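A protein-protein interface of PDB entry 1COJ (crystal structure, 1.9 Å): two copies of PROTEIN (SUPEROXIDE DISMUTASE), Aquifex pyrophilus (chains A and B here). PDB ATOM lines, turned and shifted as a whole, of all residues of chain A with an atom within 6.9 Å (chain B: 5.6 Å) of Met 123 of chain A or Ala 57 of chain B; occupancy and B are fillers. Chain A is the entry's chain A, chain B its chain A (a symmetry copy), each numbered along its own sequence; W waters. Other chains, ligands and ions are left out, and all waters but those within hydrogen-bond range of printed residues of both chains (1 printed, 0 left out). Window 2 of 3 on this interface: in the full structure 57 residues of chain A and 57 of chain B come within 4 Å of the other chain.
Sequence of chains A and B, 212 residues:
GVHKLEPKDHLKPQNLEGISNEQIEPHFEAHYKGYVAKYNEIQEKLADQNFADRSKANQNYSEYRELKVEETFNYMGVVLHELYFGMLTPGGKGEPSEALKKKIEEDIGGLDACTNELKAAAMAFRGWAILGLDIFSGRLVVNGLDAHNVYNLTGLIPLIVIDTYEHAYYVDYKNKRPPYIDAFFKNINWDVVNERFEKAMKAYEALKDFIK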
ATOM      1  N   GLU A 117     -27.039   9.692  -1.592  1.00  0.00           N
ATOM      2  CA  GLU A 117     -27.472   8.306  -1.541  1.00  0.00           C
ATOM      3  C   GLU A 117     -27.712   7.765  -2.946  1.00  0.00           C
ATOM      4  O   GLU A 117     -27.306   6.643  -3.264  1.00  0.00           O
ATOM      5  CB  GLU A 117     -28.742   8.182  -0.700  1.00  0.00           C
ATOM      6  CG  GLU A 117     -29.035   6.770  -0.203  1.00  0.00           C
ATOM      7  CD  GLU A 117     -27.981   6.239   0.762  1.00  0.00           C
ATOM      8  OE1 GLU A 117     -27.890   5.007   0.920  1.00  0.00           O
ATOM      9  OE2 GLU A 117     -27.246   7.045   1.368  1.00  0.00           O
ATOM     10  N   LEU A 118     -28.358   8.565  -3.793  1.00  0.00           N
ATOM     11  CA  LEU A 118     -28.636   8.150  -5.162  1.00  0.00           C
ATOM     12  C   LEU A 118     -27.367   7.979  -5.979  1.00  0.00           C
ATOM     13  O   LEU A 118     -27.232   7.002  -6.716  1.00  0.00           O
ATOM     14  CB  LEU A 118     -29.583   9.130  -5.862  1.00  0.00           C
ATOM     15  CG  LEU A 118     -31.072   8.778  -5.823  1.00  0.00           C
ATOM     16  CD1 LEU A 118     -31.879   9.875  -6.510  1.00  0.00           C
ATOM     17  CD2 LEU A 118     -31.307   7.425  -6.499  1.00  0.00           C
ATOM     18  N   LYS A 119     -26.438   8.924  -5.847  1.00  0.00           N
ATOM     19  CA  LYS A 119     -25.179   8.852  -6.582  1.00  0.00           C
ATOM     20  C   LYS A 119     -24.399   7.618  -6.143  1.00  0.00           C
ATOM     21  O   LYS A 119     -23.814   6.918  -6.969  1.00  0.00           O
ATOM     22  CB  LYS A 119     -24.336  10.110  -6.360  1.00  0.00           C
ATOM     23  CG  LYS A 119     -24.944  11.390  -6.908  1.00  0.00           C
ATOM     24  CD  LYS A 119     -23.983  12.552  -6.704  1.00  0.00           C
ATOM     25  CE  LYS A 119     -24.593  13.889  -7.097  1.00  0.00           C
ATOM     26  NZ  LYS A 119     -24.976  13.981  -8.532  1.00  0.00           N
ATOM     27  N   ALA A 120     -24.434   7.332  -4.846  1.00  0.00           N
ATOM     28  CA  ALA A 120     -23.738   6.175  -4.292  1.00  0.00           C
ATOM     29  C   ALA A 120     -24.299   4.870  -4.864  1.00  0.00           C
ATOM     30  O   ALA A 120     -23.538   4.001  -5.305  1.00  0.00           O
ATOM     31  CB  ALA A 120     -23.843   6.178  -2.773  1.00  0.00           C
ATOM     32  N   ALA A 121     -25.626   4.750  -4.875  1.00  0.00           N
ATOM     33  CA  ALA A 121     -26.290   3.562  -5.405  1.00  0.00           C
ATOM     34  C   ALA A 121     -25.990   3.412  -6.892  1.00  0.00           C
ATOM     35  O   ALA A 121     -25.765   2.304  -7.377  1.00  0.00           O
ATOM     36  CB  ALA A 121     -27.800   3.631  -5.164  1.00  0.00           C
ATOM     37  N   ALA A 122     -25.956   4.535  -7.608  1.00  0.00           N
ATOM     38  CA  ALA A 122     -25.667   4.523  -9.040  1.00  0.00           C
ATOM     39  C   ALA A 122     -24.239   4.051  -9.309  1.00  0.00           C
ATOM     40  O   ALA A 122     -23.961   3.431 -10.336  1.00  0.00           O
ATOM     41  CB  ALA A 122     -25.894   5.906  -9.638  1.00  0.00           C
ATOM     42  N   MET A 123     -23.333   4.357  -8.388  1.00  0.00           N
ATOM     43  CA  MET A 123     -21.941   3.942  -8.523  1.00  0.00           C
ATOM     44  C   MET A 123     -21.726   2.501  -8.053  1.00  0.00           C
ATOM     45  O   MET A 123     -20.825   1.816  -8.530  1.00  0.00           O
ATOM     46  CB  MET A 123     -21.023   4.875  -7.724  1.00  0.00           C
ATOM     47  CG  MET A 123     -20.789   6.246  -8.358  1.00  0.00           C
ATOM     48  SD  MET A 123     -20.006   6.144  -9.985  1.00  0.00           S
ATOM     49  CE  MET A 123     -18.384   5.624  -9.561  1.00  0.00           C
ATOM     50  N   ALA A 124     -22.557   2.055  -7.114  1.00  0.00           N
ATOM     51  CA  ALA A 124     -22.445   0.712  -6.546  1.00  0.00           C
ATOM     52  C   ALA A 124     -23.161  -0.391  -7.314  1.00  0.00           C
ATOM     53  O   ALA A 124     -22.831  -1.568  -7.143  1.00  0.00           O
ATOM     54  CB  ALA A 124     -22.924   0.722  -5.091  1.00  0.00           C
ATOM     55  N   PHE A 125     -24.135  -0.028  -8.146  1.00  0.00           N
ATOM     56  CA  PHE A 125     -24.886  -1.027  -8.895  1.00  0.00           C
ATOM     57  C   PHE A 125     -24.643  -1.145 -10.385  1.00  0.00           C
ATOM     58  O   PHE A 125     -24.403  -0.164 -11.083  1.00  0.00           O
ATOM     59  CB  PHE A 125     -26.366  -0.961  -8.541  1.00  0.00           C
ATOM     60  CG  PHE A 125     -26.641  -1.473  -7.167  1.00  0.00           C
ATOM     61  CD1 PHE A 125     -26.936  -2.820  -6.956  1.00  0.00           C
ATOM     62  CD2 PHE A 125     -26.493  -0.637  -6.067  1.00  0.00           C
ATOM     63  CE1 PHE A 125     -27.069  -3.322  -5.667  1.00  0.00           C
ATOM     64  CE2 PHE A 125     -26.622  -1.123  -4.779  1.00  0.00           C
ATOM     65  CZ  PHE A 125     -26.910  -2.469  -4.576  1.00  0.00           C
ATOM     66  N   ARG A 126     -24.708  -2.384 -10.854  1.00  0.00           N
ATOM     67  CA  ARG A 126     -24.428  -2.727 -12.237  1.00  0.00           C
ATOM     68  C   ARG A 126     -25.558  -2.558 -13.241  1.00  0.00           C
ATOM     69  O   ARG A 126     -25.327  -2.692 -14.445  1.00  0.00           O
ATOM     70  CB  ARG A 126     -23.887  -4.157 -12.282  1.00  0.00           C
ATOM     71  CG  ARG A 126     -22.717  -4.362 -11.324  1.00  0.00           C
ATOM     72  CD  ARG A 126     -22.379  -5.827 -11.083  1.00  0.00           C
ATOM     73  NE  ARG A 126     -21.351  -5.946 -10.048  1.00  0.00           N
ATOM     74  CZ  ARG A 126     -20.970  -7.087  -9.478  1.00  0.00           C
ATOM     75  NH1 ARG A 126     -21.525  -8.239  -9.828  1.00  0.00           N
ATOM     76  NH2 ARG A 126     -20.035  -7.071  -8.540  1.00  0.00           N
ATOM     77  N   ALA A 129     -30.347   2.369 -10.453  1.00  0.00           N
ATOM     78  CA  ALA A 129     -30.406   2.949  -9.116  1.00  0.00           C
ATOM     79  C   ALA A 129     -31.789   3.595  -9.103  1.00  0.00           C
ATOM     80  O   ALA A 129     -32.107   4.415  -9.971  1.00  0.00           O
ATOM     81  CB  ALA A 129     -29.320   3.992  -8.920  1.00  0.00           C
ATOM     82  N   THR A 164     -27.695   2.471 -15.144  1.00  0.00           N
ATOM     83  CA  THR A 164     -26.249   2.400 -14.975  1.00  0.00           C
ATOM     84  C   THR A 164     -25.614   1.369 -15.903  1.00  0.00           C
ATOM     85  O   THR A 164     -24.437   1.046 -15.770  1.00  0.00           O
ATOM     86  CB  THR A 164     -25.824   2.153 -13.498  1.00  0.00           C
ATOM     87  OG1 THR A 164     -26.314   0.887 -13.048  1.00  0.00           O
ATOM     88  CG2 THR A 164     -26.362   3.250 -12.595  1.00  0.00           C
ATOM     89  N   LYS A 176     -16.152   6.455 -17.592  1.00  0.00           N
ATOM     90  CA  LYS A 176     -16.451   7.461 -16.570  1.00  0.00           C
ATOM     91  C   LYS A 176     -17.928   7.647 -16.224  1.00  0.00           C
ATOM     92  O   LYS A 176     -18.612   8.495 -16.801  1.00  0.00           O
ATOM     93  CB  LYS A 176     -15.847   8.807 -16.973  1.00  0.00           C
ATOM     94  CG  LYS A 176     -14.354   8.750 -17.250  1.00  0.00           C
ATOM     95  CD  LYS A 176     -13.815  10.089 -17.747  1.00  0.00           C
ATOM     96  CE  LYS A 176     -14.379  10.482 -19.120  1.00  0.00           C
ATOM     97  NZ  LYS A 176     -13.946   9.566 -20.224  1.00  0.00           N
ATOM     98  N   ARG A 177     -18.381   6.927 -15.203  1.00  0.00           N
ATOM     99  CA  ARG A 177     -19.772   7.000 -14.763  1.00  0.00           C
ATOM    100  C   ARG A 177     -20.162   8.264 -13.975  1.00  0.00           C
ATOM    101  O   ARG A 177     -21.246   8.809 -14.183  1.00  0.00           O
ATOM    102  CB  ARG A 177     -20.145   5.738 -13.969  1.00  0.00           C
ATOM    103  CG  ARG A 177     -21.629   5.624 -13.648  1.00  0.00           C
ATOM    104  CD  ARG A 177     -21.955   4.347 -12.894  1.00  0.00           C
ATOM    105  NE  ARG A 177     -21.741   3.147 -13.703  1.00  0.00           N
ATOM    106  CZ  ARG A 177     -21.924   1.904 -13.265  1.00  0.00           C
ATOM    107  NH1 ARG A 177     -22.335   1.685 -12.020  1.00  0.00           N
ATOM    108  NH2 ARG A 177     -21.683   0.874 -14.068  1.00  0.00           N
ATOM    109  N   PRO A 178     -19.287   8.753 -13.073  1.00  0.00           N
ATOM    110  CA  PRO A 178     -19.621   9.959 -12.291  1.00  0.00           C
ATOM    111  C   PRO A 178     -20.118  11.177 -13.083  1.00  0.00           C
ATOM    112  O   PRO A 178     -21.138  11.776 -12.724  1.00  0.00           O
ATOM    113  CB  PRO A 178     -18.324  10.246 -11.542  1.00  0.00           C
ATOM    114  CG  PRO A 178     -17.795   8.882 -11.287  1.00  0.00           C
ATOM    115  CD  PRO A 178     -18.007   8.184 -12.613  1.00  0.00           C
ATOM    116  N   PRO A 179     -19.405  11.578 -14.150  1.00  0.00           N
ATOM    117  CA  PRO A 179     -19.882  12.738 -14.904  1.00  0.00           C
ATOM    118  C   PRO A 179     -21.245  12.489 -15.549  1.00  0.00           C
ATOM    119  O   PRO A 179     -22.018  13.425 -15.746  1.00  0.00           O
ATOM    120  CB  PRO A 179     -18.778  12.961 -15.940  1.00  0.00           C
ATOM    121  CG  PRO A 179     -18.162  11.609 -16.095  1.00  0.00           C
ATOM    122  CD  PRO A 179     -18.116  11.103 -14.689  1.00  0.00           C
ATOM    123  N   ILE A 181     -23.674  10.646 -14.185  1.00  0.00           N
ATOM    124  CA  ILE A 181     -24.658  10.777 -13.116  1.00  0.00           C
ATOM    125  C   ILE A 181     -24.972  12.256 -12.882  1.00  0.00           C
ATOM    126  O   ILE A 181     -26.132  12.632 -12.711  1.00  0.00           O
ATOM    127  CB  ILE A 181     -24.166  10.116 -11.810  1.00  0.00           C
ATOM    128  CG1 ILE A 181     -23.900   8.625 -12.050  1.00  0.00           C
ATOM    129  CG2 ILE A 181     -25.207  10.285 -10.711  1.00  0.00           C
ATOM    130  CD1 ILE A 181     -23.161   7.931 -10.917  1.00  0.00           C
ATOM    131  N   ASP B  53     -19.184   3.571   3.887  1.00  0.00           N
ATOM    132  CA  ASP B  53     -18.756   4.838   3.330  1.00  0.00           C
ATOM    133  C   ASP B  53     -19.315   5.028   1.925  1.00  0.00           C
ATOM    134  O   ASP B  53     -18.904   4.344   0.987  1.00  0.00           O
ATOM    135  CB  ASP B  53     -17.231   4.914   3.312  1.00  0.00           C
ATOM    136  CG  ASP B  53     -16.722   6.319   3.038  1.00  0.00           C
ATOM    137  OD1 ASP B  53     -17.479   7.135   2.477  1.00  0.00           O
ATOM    138  OD2 ASP B  53     -15.567   6.617   3.395  1.00  0.00           O
ATOM    139  N   ARG B  54     -20.212   5.996   1.782  1.00  0.00           N
ATOM    140  CA  ARG B  54     -20.834   6.282   0.496  1.00  0.00           C
ATOM    141  C   ARG B  54     -19.860   6.786  -0.562  1.00  0.00           C
ATOM    142  O   ARG B  54     -20.044   6.516  -1.747  1.00  0.00           O
ATOM    143  CB  ARG B  54     -21.991   7.267   0.668  1.00  0.00           C
ATOM    144  CG  ARG B  54     -23.363   6.633   0.489  1.00  0.00           C
ATOM    145  CD  ARG B  54     -24.218   6.668   1.746  1.00  0.00           C
ATOM    146  NE  ARG B  54     -23.765   5.763   2.797  1.00  0.00           N
ATOM    147  CZ  ARG B  54     -24.575   5.090   3.614  1.00  0.00           C
ATOM    148  NH1 ARG B  54     -25.894   5.196   3.508  1.00  0.00           N
ATOM    149  NH2 ARG B  54     -24.065   4.341   4.576  1.00  0.00           N
ATOM    150  N   SER B  55     -18.806   7.481  -0.138  1.00  0.00           N
ATOM    151  CA  SER B  55     -17.826   8.002  -1.085  1.00  0.00           C
ATOM    152  C   SER B  55     -16.995   6.894  -1.713  1.00  0.00           C
ATOM    153  O   SER B  55     -16.362   7.100  -2.743  1.00  0.00           O
ATOM    154  CB  SER B  55     -16.907   9.036  -0.427  1.00  0.00           C
ATOM    155  OG  SER B  55     -16.082   8.449   0.561  1.00  0.00           O
ATOM    156  N   LYS B  56     -17.001   5.720  -1.089  1.00  0.00           N
ATOM    157  CA  LYS B  56     -16.251   4.579  -1.602  1.00  0.00           C
ATOM    158  C   LYS B  56     -17.128   3.627  -2.416  1.00  0.00           C
ATOM    159  O   LYS B  56     -16.685   2.542  -2.783  1.00  0.00           O
ATOM    160  CB  LYS B  56     -15.599   3.807  -0.456  1.00  0.00           C
ATOM    161  CG  LYS B  56     -14.489   4.553   0.259  1.00  0.00           C
ATOM    162  CD  LYS B  56     -13.880   3.684   1.351  1.00  0.00           C
ATOM    163  CE  LYS B  56     -12.695   4.358   2.027  1.00  0.00           C
ATOM    164  NZ  LYS B  56     -13.059   5.679   2.613  1.00  0.00           N
ATOM    165  N   ALA B  57     -18.378   4.013  -2.650  1.00  0.00           N
ATOM    166  CA  ALA B  57     -19.308   3.193  -3.422  1.00  0.00           C
ATOM    167  C   ALA B  57     -18.669   2.762  -4.744  1.00  0.00           C
ATOM    168  O   ALA B  57     -18.193   3.593  -5.525  1.00  0.00           O
ATOM    169  CB  ALA B  57     -20.605   3.960  -3.668  1.00  0.00           C
ATOM    170  N   ASN B  58     -18.644   1.452  -4.972  1.00  0.00           N
ATOM    171  CA  ASN B  58     -18.037   0.879  -6.166  1.00  0.00           C
ATOM    172  C   ASN B  58     -18.771  -0.417  -6.511  1.00  0.00           C
ATOM    173  O   ASN B  58     -19.086  -1.211  -5.621  1.00  0.00           O
ATOM    174  CB  ASN B  58     -16.553   0.611  -5.891  1.00  0.00           C
ATOM    175  CG  ASN B  58     -15.827   0.056  -7.092  1.00  0.00           C
ATOM    176  OD1 ASN B  58     -15.834  -1.150  -7.326  1.00  0.00           O
ATOM    177  ND2 ASN B  58     -15.208   0.932  -7.868  1.00  0.00           N
ATOM    178  N   GLN B  59     -19.025  -0.633  -7.801  1.00  0.00           N
ATOM    179  CA  GLN B  59     -19.754  -1.814  -8.257  1.00  0.00           C
ATOM    180  C   GLN B  59     -18.997  -3.136  -8.244  1.00  0.00           C
ATOM    181  O   GLN B  59     -19.612  -4.189  -8.375  1.00  0.00           O
ATOM    182  CB  GLN B  59     -20.355  -1.581  -9.649  1.00  0.00           C
ATOM    183  CG  GLN B  59     -19.332  -1.400 -10.762  1.00  0.00           C
ATOM    184  CD  GLN B  59     -19.937  -1.553 -12.149  1.00  0.00           C
ATOM    185  OE1 GLN B  59     -19.229  -1.868 -13.107  1.00  0.00           O
ATOM    186  NE2 GLN B  59     -21.242  -1.344 -12.266  1.00  0.00           N
ATOM    187  N   SER B  62     -17.594  -2.907  -2.467  1.00  0.00           N
ATOM    188  CA  SER B  62     -17.606  -1.797  -1.518  1.00  0.00           C
ATOM    189  C   SER B  62     -18.566  -2.203  -0.401  1.00  0.00           C
ATOM    190  O   SER B  62     -19.554  -2.902  -0.656  1.00  0.00           O
ATOM    191  CB  SER B  62     -18.041  -0.480  -2.178  1.00  0.00           C
ATOM    192  OG  SER B  62     -19.310  -0.581  -2.794  1.00  0.00           O
ATOM    193  N   TYR B  64     -20.690  -0.505   1.162  1.00  0.00           N
ATOM    194  CA  TYR B  64     -22.007   0.040   0.859  1.00  0.00           C
ATOM    195  C   TYR B  64     -22.791  -0.860  -0.098  1.00  0.00           C
ATOM    196  O   TYR B  64     -23.966  -1.163   0.138  1.00  0.00           O
ATOM    197  CB  TYR B  64     -21.878   1.441   0.260  1.00  0.00           C
ATOM    198  CG  TYR B  64     -23.200   2.039  -0.158  1.00  0.00           C
ATOM    199  CD1 TYR B  64     -24.113   2.493   0.793  1.00  0.00           C
ATOM    200  CD2 TYR B  64     -23.550   2.131  -1.503  1.00  0.00           C
ATOM    201  CE1 TYR B  64     -25.342   3.018   0.412  1.00  0.00           C
ATOM    202  CE2 TYR B  64     -24.779   2.657  -1.893  1.00  0.00           C
ATOM    203  CZ  TYR B  64     -25.669   3.093  -0.935  1.00  0.00           C
ATOM    204  OH  TYR B  64     -26.902   3.564  -1.327  1.00  0.00           O
HETATM  205  O   HOH W   1     -18.345   1.567  -9.736  1.00  0.00           O
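Water W1 bridges O of Met 123 of chain A and N of Gln 59 of chain B.
Of the 9 printed residues of chain B, 5 touch a printed residue of chain A.
Hydrophobic or aromatic side chains of chain B within 4 Å of the printed part of chain A: Ala 57 and Tyr 64.
Of the 17 printed residues of chain A, 8 touch a printed residue of chain B.
Hydrophobic or aromatic side chains of chain A within 4 Å of the printed part of chain B: Ala 120, Ala 121, Met 123 and Ala 124.
Among the printed residues, 15 pairs touch across the chains.
Among the printed residues, Asp or Glu carboxylates within 4 Å of a Lys or Arg side-chain nitrogen of the other chain: Glu 117 of chain A with Arg 54 of chain B.
The side-chain carboxylate (OE2) of Glu 117 of chain A is in salt-bridge range of the guanidinium group (NH1) of Arg 54 of chain B, at 3.1 Å.
OH of Tyr 64 of chain B lies within hydrogen-bond range of OE1 of Glu 117 of chain A (2.8 Å).
The backbone NH (N) of Gln 59 of chain B is in hydrogen-bond range of the backbone carbonyl oxygen (O) of Met 123 of chain A (3.1 Å).
NH2 of Arg 126 of chain A is in hydrogen-bond range of O of Gln 59 of chain B.
NH2 of Arg 177 of chain A lies close to NE2 of Gln 59 of chain B (2.9 Å).
Of chain B, only Ala 57 (3.8 Å), Asn 58 (3.6 Å) and Gln 59 (3.1 Å) come within 4 Å of Met 123 of chain A.
Ala 57 of chain B touches just these residues of chain A: Ala 120 and Met 123.
Of the printed residues of chain B, Phe 125 of chain A touches Gln 59 (3.6 Å).
Of the printed residues of chain B, Ala 124 of chain A touches Asn 58, Gln 59 and Tyr 64.
Ser 62 of chain B touches none of the printed residues of chain A.
The nearest residue of chain A that does not touch Ala 57 of chain B is Ala 124 of chain A (4.2 Å).
O of Ala 122 of chain A is in hydrogen-bond range of NH1 of Arg 177 of chain A (2.9 Å).
The backbone carbonyl oxygen of Phe 125 of chain A is in hydrogen-bond range of the side-chain hydroxyl of Thr 164 of chain A (2.9 Å).
O of Phe 125 of chain A is in hydrogen-bond range of NH1 of Arg 177 of chain A, 2.9 Å away.
O of Thr 164 of chain A sits at hydrogen-bond distance from NH2 of Arg 177 of chain A (3.2 Å).
O of Asn 58 of chain B lies within hydrogen-bond range of OG of Ser 62 of chain B (2.9 Å).
Ala 120 of chain A touches Arg 54 of chain B (CB to CG, 3.3 Å).
Ala 57 of chain B touches Ala 120 of chain A (CB to O, 3.4 Å).
CE2 of Tyr 64 of chain B touches C of Ala 120 of chain A, at 3.7 Å.
N of Ala 121 of chain A touches CE2 of Tyr 64 of chain B, 3.7 Å away.
Ala 57 of chain B touches Met 123 of chain A (O to CB, 3.8 Å).
O of Met 123 of chain A touches C of Asn 58 of chain B (3.6 Å).
C of Asn 58 of chain B touches CA of Ala 124 of chain A (3.8 Å).
CA of Gln 59 of chain B touches O of Ala 124 of chain A (3.3 Å).
CB of Ala 124 of chain A touches CD2 of Tyr 64 of chain B, at 3.9 Å.
Phe 125 of chain A touches Gln 59 of chain B.
No position is printed for both chains.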
